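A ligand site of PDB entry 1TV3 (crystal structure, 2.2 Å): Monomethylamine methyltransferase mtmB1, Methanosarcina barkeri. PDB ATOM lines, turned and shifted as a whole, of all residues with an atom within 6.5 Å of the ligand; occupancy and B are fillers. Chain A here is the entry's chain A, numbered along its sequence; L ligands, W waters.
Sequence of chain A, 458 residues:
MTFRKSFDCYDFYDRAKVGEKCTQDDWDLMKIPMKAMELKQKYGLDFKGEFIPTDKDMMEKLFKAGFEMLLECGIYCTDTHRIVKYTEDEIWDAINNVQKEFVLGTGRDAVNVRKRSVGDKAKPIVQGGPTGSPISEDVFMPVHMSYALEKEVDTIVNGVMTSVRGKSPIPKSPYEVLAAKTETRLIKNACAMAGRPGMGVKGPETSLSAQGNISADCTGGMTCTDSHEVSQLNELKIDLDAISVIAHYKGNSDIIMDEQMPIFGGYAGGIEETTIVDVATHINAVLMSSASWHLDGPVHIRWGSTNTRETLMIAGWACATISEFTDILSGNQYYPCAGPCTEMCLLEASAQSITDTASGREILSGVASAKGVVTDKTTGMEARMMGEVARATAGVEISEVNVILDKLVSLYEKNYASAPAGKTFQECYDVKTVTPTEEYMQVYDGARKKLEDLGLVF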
ATOM      1  N   GLN A 127      -3.285 -13.190 -27.169  1.00  0.00           N
ATOM      2  CA  GLN A 127      -3.232 -14.465 -27.872  1.00  0.00           C
ATOM      3  C   GLN A 127      -4.561 -14.655 -28.584  1.00  0.00           C
ATOM      4  O   GLN A 127      -5.569 -14.971 -27.951  1.00  0.00           O
ATOM      5  CB  GLN A 127      -2.991 -15.603 -26.884  1.00  0.00           C
ATOM      6  CG  GLN A 127      -2.778 -16.951 -27.545  1.00  0.00           C
ATOM      7  CD  GLN A 127      -2.032 -17.922 -26.644  1.00  0.00           C
ATOM      8  OE1 GLN A 127      -2.619 -18.575 -25.782  1.00  0.00           O
ATOM      9  NE2 GLN A 127      -0.716 -17.989 -26.828  1.00  0.00           N
ATOM     10  N   PRO A 130      -9.071 -19.114 -33.025  1.00  0.00           N
ATOM     11  CA  PRO A 130     -10.379 -19.752 -32.861  1.00  0.00           C
ATOM     12  C   PRO A 130     -10.573 -20.273 -31.449  1.00  0.00           C
ATOM     13  O   PRO A 130     -11.665 -20.681 -31.063  1.00  0.00           O
ATOM     14  CB  PRO A 130     -10.335 -20.861 -33.904  1.00  0.00           C
ATOM     15  CG  PRO A 130      -9.498 -20.258 -34.999  1.00  0.00           C
ATOM     16  CD  PRO A 130      -8.370 -19.646 -34.204  1.00  0.00           C
ATOM     17  N   THR A 131      -9.487 -20.278 -30.679  1.00  0.00           N
ATOM     18  CA  THR A 131      -9.530 -20.714 -29.289  1.00  0.00           C
ATOM     19  C   THR A 131     -10.176 -22.098 -29.141  1.00  0.00           C
ATOM     20  O   THR A 131     -11.146 -22.278 -28.399  1.00  0.00           O
ATOM     21  CB  THR A 131     -10.307 -19.673 -28.445  1.00  0.00           C
ATOM     22  OG1 THR A 131      -9.855 -18.362 -28.793  1.00  0.00           O
ATOM     23  CG2 THR A 131     -10.055 -19.883 -26.964  1.00  0.00           C
ATOM     24  N   GLY A 132      -9.620 -23.078 -29.858  1.00  0.00           N
ATOM     25  CA  GLY A 132     -10.104 -24.443 -29.778  1.00  0.00           C
ATOM     26  C   GLY A 132     -11.423 -24.761 -30.455  1.00  0.00           C
ATOM     27  O   GLY A 132     -11.901 -25.886 -30.370  1.00  0.00           O
ATOM     28  N   SER A 133     -12.017 -23.781 -31.133  1.00  0.00           N
ATOM     29  CA  SER A 133     -13.291 -24.010 -31.799  1.00  0.00           C
ATOM     30  C   SER A 133     -13.119 -24.757 -33.116  1.00  0.00           C
ATOM     31  O   SER A 133     -12.079 -24.668 -33.767  1.00  0.00           O
ATOM     32  CB  SER A 133     -13.985 -22.670 -32.056  1.00  0.00           C
ATOM     33  OG  SER A 133     -14.138 -21.946 -30.844  1.00  0.00           O
ATOM     34  N   VAL A 157      -3.839 -18.793 -30.779  1.00  0.00           N
ATOM     35  CA  VAL A 157      -4.351 -19.932 -30.022  1.00  0.00           C
ATOM     36  C   VAL A 157      -5.085 -20.744 -31.097  1.00  0.00           C
ATOM     37  O   VAL A 157      -6.085 -20.299 -31.671  1.00  0.00           O
ATOM     38  CB  VAL A 157      -5.325 -19.558 -28.865  1.00  0.00           C
ATOM     39  CG1 VAL A 157      -6.365 -18.540 -29.323  1.00  0.00           C
ATOM     40  CG2 VAL A 157      -6.004 -20.823 -28.362  1.00  0.00           C
ATOM     41  N   ASN A 158      -4.577 -21.947 -31.360  1.00  0.00           N
ATOM     42  CA  ASN A 158      -5.110 -22.832 -32.391  1.00  0.00           C
ATOM     43  C   ASN A 158      -6.582 -23.223 -32.333  1.00  0.00           C
ATOM     44  O   ASN A 158      -7.171 -23.353 -31.259  1.00  0.00           O
ATOM     45  CB  ASN A 158      -4.291 -24.124 -32.437  1.00  0.00           C
ATOM     46  CG  ASN A 158      -2.812 -23.881 -32.680  1.00  0.00           C
ATOM     47  OD1 ASN A 158      -2.373 -22.729 -32.852  1.00  0.00           O
ATOM     48  ND2 ASN A 158      -2.033 -24.955 -32.701  1.00  0.00           N
ATOM     49  N   LYS A 202      -0.397 -21.802 -29.579  1.00  0.00           N
ATOM     50  CA  LYS A 202      -0.773 -22.533 -28.382  1.00  0.00           C
ATOM     51  C   LYS A 202      -1.632 -23.696 -28.822  1.00  0.00           C
ATOM     52  O   LYS A 202      -2.640 -23.513 -29.513  1.00  0.00           O
ATOM     53  CB  LYS A 202      -1.542 -21.618 -27.406  1.00  0.00           C
ATOM     54  CG  LYS A 202      -1.771 -22.257 -26.047  1.00  0.00           C
ATOM     55  CD  LYS A 202      -3.150 -22.905 -25.926  1.00  0.00           C
ATOM     56  CE  LYS A 202      -4.199 -21.889 -25.463  1.00  0.00           C
ATOM     57  NZ  LYS A 202      -5.507 -22.502 -25.101  1.00  0.00           N
ATOM     58  N   GLY A 203      -1.226 -24.899 -28.436  1.00  0.00           N
ATOM     59  CA  GLY A 203      -1.945 -26.108 -28.779  1.00  0.00           C
ATOM     60  C   GLY A 203      -1.192 -27.286 -28.180  1.00  0.00           C
ATOM     61  O   GLY A 203      -0.466 -27.093 -27.208  1.00  0.00           O
ATOM     62  N   PRO A 204      -1.335 -28.513 -28.735  1.00  0.00           N
ATOM     63  CA  PRO A 204      -2.139 -28.913 -29.906  1.00  0.00           C
ATOM     64  C   PRO A 204      -3.613 -29.079 -29.503  1.00  0.00           C
ATOM     65  O   PRO A 204      -3.917 -29.669 -28.474  1.00  0.00           O
ATOM     66  CB  PRO A 204      -1.490 -30.219 -30.324  1.00  0.00           C
ATOM     67  CG  PRO A 204      -1.126 -30.839 -29.001  1.00  0.00           C
ATOM     68  CD  PRO A 204      -0.580 -29.663 -28.194  1.00  0.00           C
ATOM     69  N   GLU A 205      -4.522 -28.581 -30.339  1.00  0.00           N
ATOM     70  CA  GLU A 205      -5.936 -28.642 -30.010  1.00  0.00           C
ATOM     71  C   GLU A 205      -6.778 -29.755 -30.615  1.00  0.00           C
ATOM     72  O   GLU A 205      -7.663 -30.291 -29.948  1.00  0.00           O
ATOM     73  CB  GLU A 205      -6.590 -27.292 -30.323  1.00  0.00           C
ATOM     74  CG  GLU A 205      -5.952 -26.106 -29.613  1.00  0.00           C
ATOM     75  CD  GLU A 205      -5.868 -26.286 -28.103  1.00  0.00           C
ATOM     76  OE1 GLU A 205      -6.780 -26.932 -27.525  1.00  0.00           O
ATOM     77  OE2 GLU A 205      -4.905 -25.774 -27.499  1.00  0.00           O
ATOM     78  N   GLU A 229      -0.228 -27.178 -24.331  1.00  0.00           N
ATOM     79  CA  GLU A 229      -1.365 -27.368 -23.445  1.00  0.00           C
ATOM     80  C   GLU A 229      -1.545 -28.717 -22.785  1.00  0.00           C
ATOM     81  O   GLU A 229      -1.274 -29.760 -23.372  1.00  0.00           O
ATOM     82  CB  GLU A 229      -2.662 -27.005 -24.186  1.00  0.00           C
ATOM     83  CG  GLU A 229      -3.110 -28.021 -25.245  1.00  0.00           C
ATOM     84  CD  GLU A 229      -3.762 -29.274 -24.656  1.00  0.00           C
ATOM     85  OE1 GLU A 229      -4.351 -29.179 -23.549  1.00  0.00           O
ATOM     86  OE2 GLU A 229      -3.701 -30.350 -25.297  1.00  0.00           O
ATOM     87  N   VAL A 230      -1.995 -28.667 -21.538  1.00  0.00           N
ATOM     88  CA  VAL A 230      -2.330 -29.837 -20.747  1.00  0.00           C
ATOM     89  C   VAL A 230      -3.476 -29.345 -19.861  1.00  0.00           C
ATOM     90  O   VAL A 230      -3.407 -28.247 -19.303  1.00  0.00           O
ATOM     91  CB  VAL A 230      -1.145 -30.342 -19.897  1.00  0.00           C
ATOM     92  CG1 VAL A 230      -0.692 -29.277 -18.918  1.00  0.00           C
ATOM     93  CG2 VAL A 230      -1.549 -31.620 -19.181  1.00  0.00           C
ATOM     94  N   SER A 231      -4.526 -30.133 -19.748  1.00  0.00           N
ATOM     95  CA  SER A 231      -5.695 -29.729 -18.986  1.00  0.00           C
ATOM     96  C   SER A 231      -5.998 -30.462 -17.689  1.00  0.00           C
ATOM     97  O   SER A 231      -6.022 -31.688 -17.652  1.00  0.00           O
ATOM     98  CB  SER A 231      -6.954 -29.837 -19.862  1.00  0.00           C
ATOM     99  OG  SER A 231      -6.818 -29.078 -21.051  1.00  0.00           O
ATOM    100  N   MET A 257       1.817 -24.884 -20.795  1.00  0.00           N
ATOM    101  CA  MET A 257       0.656 -24.137 -20.359  1.00  0.00           C
ATOM    102  C   MET A 257      -0.350 -25.108 -19.741  1.00  0.00           C
ATOM    103  O   MET A 257      -0.937 -25.935 -20.436  1.00  0.00           O
ATOM    104  CB  MET A 257      -0.038 -23.414 -21.517  1.00  0.00           C
ATOM    105  CG  MET A 257      -1.290 -22.679 -21.040  1.00  0.00           C
ATOM    106  SD  MET A 257      -2.527 -22.354 -22.316  1.00  0.00           S
ATOM    107  CE  MET A 257      -3.310 -23.958 -22.417  1.00  0.00           C
ATOM    108  N   GLU A 259      -3.888 -25.734 -18.018  1.00  0.00           N
ATOM    109  CA  GLU A 259      -5.200 -25.092 -17.971  1.00  0.00           C
ATOM    110  C   GLU A 259      -6.142 -25.756 -16.968  1.00  0.00           C
ATOM    111  O   GLU A 259      -5.995 -26.935 -16.639  1.00  0.00           O
ATOM    112  CB  GLU A 259      -5.880 -25.150 -19.351  1.00  0.00           C
ATOM    113  CG  GLU A 259      -7.179 -25.946 -19.300  1.00  0.00           C
ATOM    114  CD  GLU A 259      -8.026 -25.820 -20.530  1.00  0.00           C
ATOM    115  OE1 GLU A 259      -8.371 -24.678 -20.904  1.00  0.00           O
ATOM    116  OE2 GLU A 259      -8.374 -26.868 -21.103  1.00  0.00           O
ATOM    117  N   MET A 261     -10.499 -24.996 -15.860  1.00  0.00           N
ATOM    118  CA  MET A 261     -11.687 -24.150 -15.953  1.00  0.00           C
ATOM    119  C   MET A 261     -12.639 -24.460 -14.802  1.00  0.00           C
ATOM    120  O   MET A 261     -13.547 -25.289 -14.939  1.00  0.00           O
ATOM    121  CB  MET A 261     -12.394 -24.385 -17.292  1.00  0.00           C
ATOM    122  CG  MET A 261     -11.550 -24.061 -18.509  1.00  0.00           C
ATOM    123  SD  MET A 261     -12.486 -24.269 -20.045  1.00  0.00           S
ATOM    124  CE  MET A 261     -13.408 -22.718 -20.111  1.00  0.00           C
ATOM    125  N   TRP A 293       3.236 -21.428 -17.364  1.00  0.00           N
ATOM    126  CA  TRP A 293       2.144 -20.501 -17.047  1.00  0.00           C
ATOM    127  C   TRP A 293       0.822 -21.259 -16.970  1.00  0.00           C
ATOM    128  O   TRP A 293       0.699 -22.353 -17.522  1.00  0.00           O
ATOM    129  CB  TRP A 293       2.055 -19.345 -18.060  1.00  0.00           C
ATOM    130  CG  TRP A 293       1.702 -19.701 -19.477  1.00  0.00           C
ATOM    131  CD1 TRP A 293       2.535 -20.229 -20.419  1.00  0.00           C
ATOM    132  CD2 TRP A 293       0.464 -19.427 -20.149  1.00  0.00           C
ATOM    133  NE1 TRP A 293       1.899 -20.302 -21.635  1.00  0.00           N
ATOM    134  CE2 TRP A 293       0.626 -19.814 -21.502  1.00  0.00           C
ATOM    135  CE3 TRP A 293      -0.773 -18.899 -19.734  1.00  0.00           C
ATOM    136  CZ2 TRP A 293      -0.406 -19.681 -22.446  1.00  0.00           C
ATOM    137  CZ3 TRP A 293      -1.795 -18.762 -20.678  1.00  0.00           C
ATOM    138  CH2 TRP A 293      -1.601 -19.153 -22.016  1.00  0.00           C
ATOM    139  N   LEU A 295      -3.412 -21.278 -17.519  1.00  0.00           N
ATOM    140  CA  LEU A 295      -4.559 -20.700 -18.194  1.00  0.00           C
ATOM    141  C   LEU A 295      -5.832 -20.983 -17.393  1.00  0.00           C
ATOM    142  O   LEU A 295      -6.185 -22.141 -17.155  1.00  0.00           O
ATOM    143  CB  LEU A 295      -4.706 -21.301 -19.596  1.00  0.00           C
ATOM    144  CG  LEU A 295      -5.919 -20.773 -20.391  1.00  0.00           C
ATOM    145  CD1 LEU A 295      -5.696 -19.306 -20.772  1.00  0.00           C
ATOM    146  CD2 LEU A 295      -6.115 -21.619 -21.628  1.00  0.00           C
ATOM    147  N   ASN A 332      -6.185 -16.127 -19.189  1.00  0.00           N
ATOM    148  CA  ASN A 332      -7.583 -16.521 -19.073  1.00  0.00           C
ATOM    149  C   ASN A 332      -8.141 -16.698 -20.495  1.00  0.00           C
ATOM    150  O   ASN A 332      -7.703 -16.007 -21.419  1.00  0.00           O
ATOM    151  CB  ASN A 332      -8.372 -15.443 -18.301  1.00  0.00           C
ATOM    152  CG  ASN A 332      -9.703 -15.959 -17.782  1.00  0.00           C
ATOM    153  OD1 ASN A 332      -9.941 -17.173 -17.744  1.00  0.00           O
ATOM    154  ND2 ASN A 332     -10.572 -15.044 -17.360  1.00  0.00           N
ATOM    155  N   GLN A 333      -9.073 -17.647 -20.662  1.00  0.00           N
ATOM    156  CA  GLN A 333      -9.652 -17.921 -21.975  1.00  0.00           C
ATOM    157  C   GLN A 333     -11.060 -17.334 -22.111  1.00  0.00           C
ATOM    158  O   GLN A 333     -11.792 -17.217 -21.122  1.00  0.00           O
ATOM    159  CB  GLN A 333      -9.667 -19.427 -22.238  1.00  0.00           C
ATOM    160  CG  GLN A 333     -10.390 -20.249 -21.202  1.00  0.00           C
ATOM    161  CD  GLN A 333     -10.018 -21.717 -21.280  1.00  0.00           C
ATOM    162  OE1 GLN A 333     -10.352 -22.408 -22.237  1.00  0.00           O
ATOM    163  NE2 GLN A 333      -9.307 -22.196 -20.266  1.00  0.00           N
ATOM    164  N   TYR A 334     -11.433 -16.987 -23.331  1.00  0.00           N
ATOM    165  CA  TYR A 334     -12.703 -16.333 -23.623  1.00  0.00           C
ATOM    166  C   TYR A 334     -13.807 -17.154 -24.282  1.00  0.00           C
ATOM    167  O   TYR A 334     -13.659 -17.602 -25.428  1.00  0.00           O
ATOM    168  CB  TYR A 334     -12.425 -15.081 -24.490  1.00  0.00           C
ATOM    169  CG  TYR A 334     -11.632 -14.016 -23.779  1.00  0.00           C
ATOM    170  CD1 TYR A 334     -10.398 -14.309 -23.177  1.00  0.00           C
ATOM    171  CD2 TYR A 334     -12.120 -12.709 -23.661  1.00  0.00           C
ATOM    172  CE1 TYR A 334      -9.692 -13.332 -22.478  1.00  0.00           C
ATOM    173  CE2 TYR A 334     -11.416 -11.726 -22.970  1.00  0.00           C
ATOM    174  CZ  TYR A 334     -10.203 -12.049 -22.374  1.00  0.00           C
ATOM    175  OH  TYR A 334      -9.530 -11.103 -21.640  1.00  0.00           O
ATOM    176  N   TYR A 335     -14.903 -17.331 -23.558  1.00  0.00           N
ATOM    177  CA  TYR A 335     -16.058 -18.064 -24.058  1.00  0.00           C
ATOM    178  C   TYR A 335     -17.346 -17.238 -23.926  1.00  0.00           C
ATOM    179  O   TYR A 335     -18.068 -17.348 -22.934  1.00  0.00           O
ATOM    180  CB  TYR A 335     -16.249 -19.382 -23.300  1.00  0.00           C
ATOM    181  CG  TYR A 335     -15.408 -20.535 -23.812  1.00  0.00           C
ATOM    182  CD1 TYR A 335     -14.079 -20.695 -23.405  1.00  0.00           C
ATOM    183  CD2 TYR A 335     -15.938 -21.464 -24.707  1.00  0.00           C
ATOM    184  CE1 TYR A 335     -13.305 -21.769 -23.858  1.00  0.00           C
ATOM    185  CE2 TYR A 335     -15.186 -22.539 -25.167  1.00  0.00           C
ATOM    186  CZ  TYR A 335     -13.873 -22.681 -24.740  1.00  0.00           C
ATOM    187  OH  TYR A 335     -13.135 -23.745 -25.201  1.00  0.00           O
ATOM    188  N   SER A 365      -6.305 -15.076 -23.908  1.00  0.00           N
ATOM    189  CA  SER A 365      -6.434 -16.071 -24.981  1.00  0.00           C
ATOM    190  C   SER A 365      -7.886 -16.213 -25.443  1.00  0.00           C
ATOM    191  O   SER A 365      -8.713 -16.833 -24.758  1.00  0.00           O
ATOM    192  CB  SER A 365      -5.900 -17.413 -24.481  1.00  0.00           C
ATOM    193  OG  SER A 365      -5.630 -18.308 -25.534  1.00  0.00           O
ATOM    194  N   GLY A 366      -8.197 -15.634 -26.600  1.00  0.00           N
ATOM    195  CA  GLY A 366      -9.551 -15.689 -27.134  1.00  0.00           C
ATOM    196  C   GLY A 366      -9.594 -15.473 -28.638  1.00  0.00           C
ATOM    197  O   GLY A 366      -8.537 -15.273 -29.250  1.00  0.00           O
ATOM    198  N   ALA A 368     -13.312 -17.640 -28.164  1.00  0.00           N
ATOM    199  CA  ALA A 368     -14.130 -18.801 -28.547  1.00  0.00           C
ATOM    200  C   ALA A 368     -15.591 -18.377 -28.621  1.00  0.00           C
ATOM    201  O   ALA A 368     -16.410 -18.764 -27.790  1.00  0.00           O
ATOM    202  CB  ALA A 368     -13.955 -19.929 -27.518  1.00  0.00           C
HETATM  203  C1  LIG L   1      -6.675 -21.850 -25.044  1.00  0.00           C
HETATM  204  C2  LIG L   1      -7.905 -22.676 -24.686  1.00  0.00           C
HETATM  205  C3  LIG L   1      -8.648 -23.164 -25.923  1.00  0.00           C
HETATM  206  C4  LIG L   1      -8.138 -24.602 -26.148  1.00  0.00           C
HETATM  207  C5  LIG L   1      -7.796 -25.152 -24.757  1.00  0.00           C
HETATM  208  C6  LIG L   1     -10.048 -23.102 -25.599  1.00  0.00           C
HETATM  209  N1  LIG L   1      -7.569 -23.934 -23.882  1.00  0.00           N
HETATM  210  O1  LIG L   1      -6.770 -20.613 -25.119  1.00  0.00           O
HETATM  211  N2  LIG L   1      -6.589 -25.925 -24.809  1.00  0.00           N
HETATM  212  O2  LIG L   1      -5.283 -25.306 -25.043  1.00  0.00           O
HETATM  213  C7  LIG L   1      -6.466 -26.702 -23.584  1.00  0.00           C
HETATM  214  O   HOH W   1     -10.673 -25.325 -22.845  1.00  0.00           O
HETATM  215  O   HOH W   2      -8.307 -28.484 -25.473  1.00  0.00           O
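NZ of Lys 202 is bonded to C1 of the ligand, 1.3 Å away.
The side-chain hydroxyl of Ser 365 lies within hydrogen-bond range of an oxygen (O1) of the ligand (2.6 Å).
A nitrogen (N1) of the ligand is in salt-bridge range of the side-chain carboxylate (OE1) of Glu 259, 3.2 Å away.
The side-chain carboxylate of Glu 205 is in hydrogen-bond range of an oxygen (O2) of the ligand, at 2.5 Å.
O of Lys 202 is in hydrogen-bond range of N of Asn 158 (3.1 Å).
O of Val 230 is in hydrogen-bond range of N of Glu 259 (2.9 Å).
O of Gly 203 is in hydrogen-bond range of N of Glu 229.
OG of Ser 365 sits at hydrogen-bond distance from OE1 of Gln 127.
The backbone NH (N) of Ser 365 sits at hydrogen-bond distance from the backbone carbonyl oxygen (O) of Asn 332.
OE1 of Gln 333 sits close to SD of Met 261 (3.6 Å).
The backbone NH (N) of Tyr 334 lies within hydrogen-bond range of the backbone carbonyl oxygen (O) of Ser 365.
O of Met 257 lies within hydrogen-bond range of N of Val 230.
Thr 131 touches the ligand.
Val 157 touches the ligand (CG2 to O1, 3.3 Å).
CB of Glu 229 touches O2 of the ligand, at 3.2 Å.
Ser 231 touches the ligand.
CE of Met 257 touches O2 of the ligand, at 3.6 Å.
Leu 295 touches the ligand (CD2 to C1, 3.5 Å).
Gln 333 touches the ligand.
Tyr 335 touches the ligand (OH to C6, 3.2 Å).
Of the 26 residues printed, 12 come within 4 Å of the ligand.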
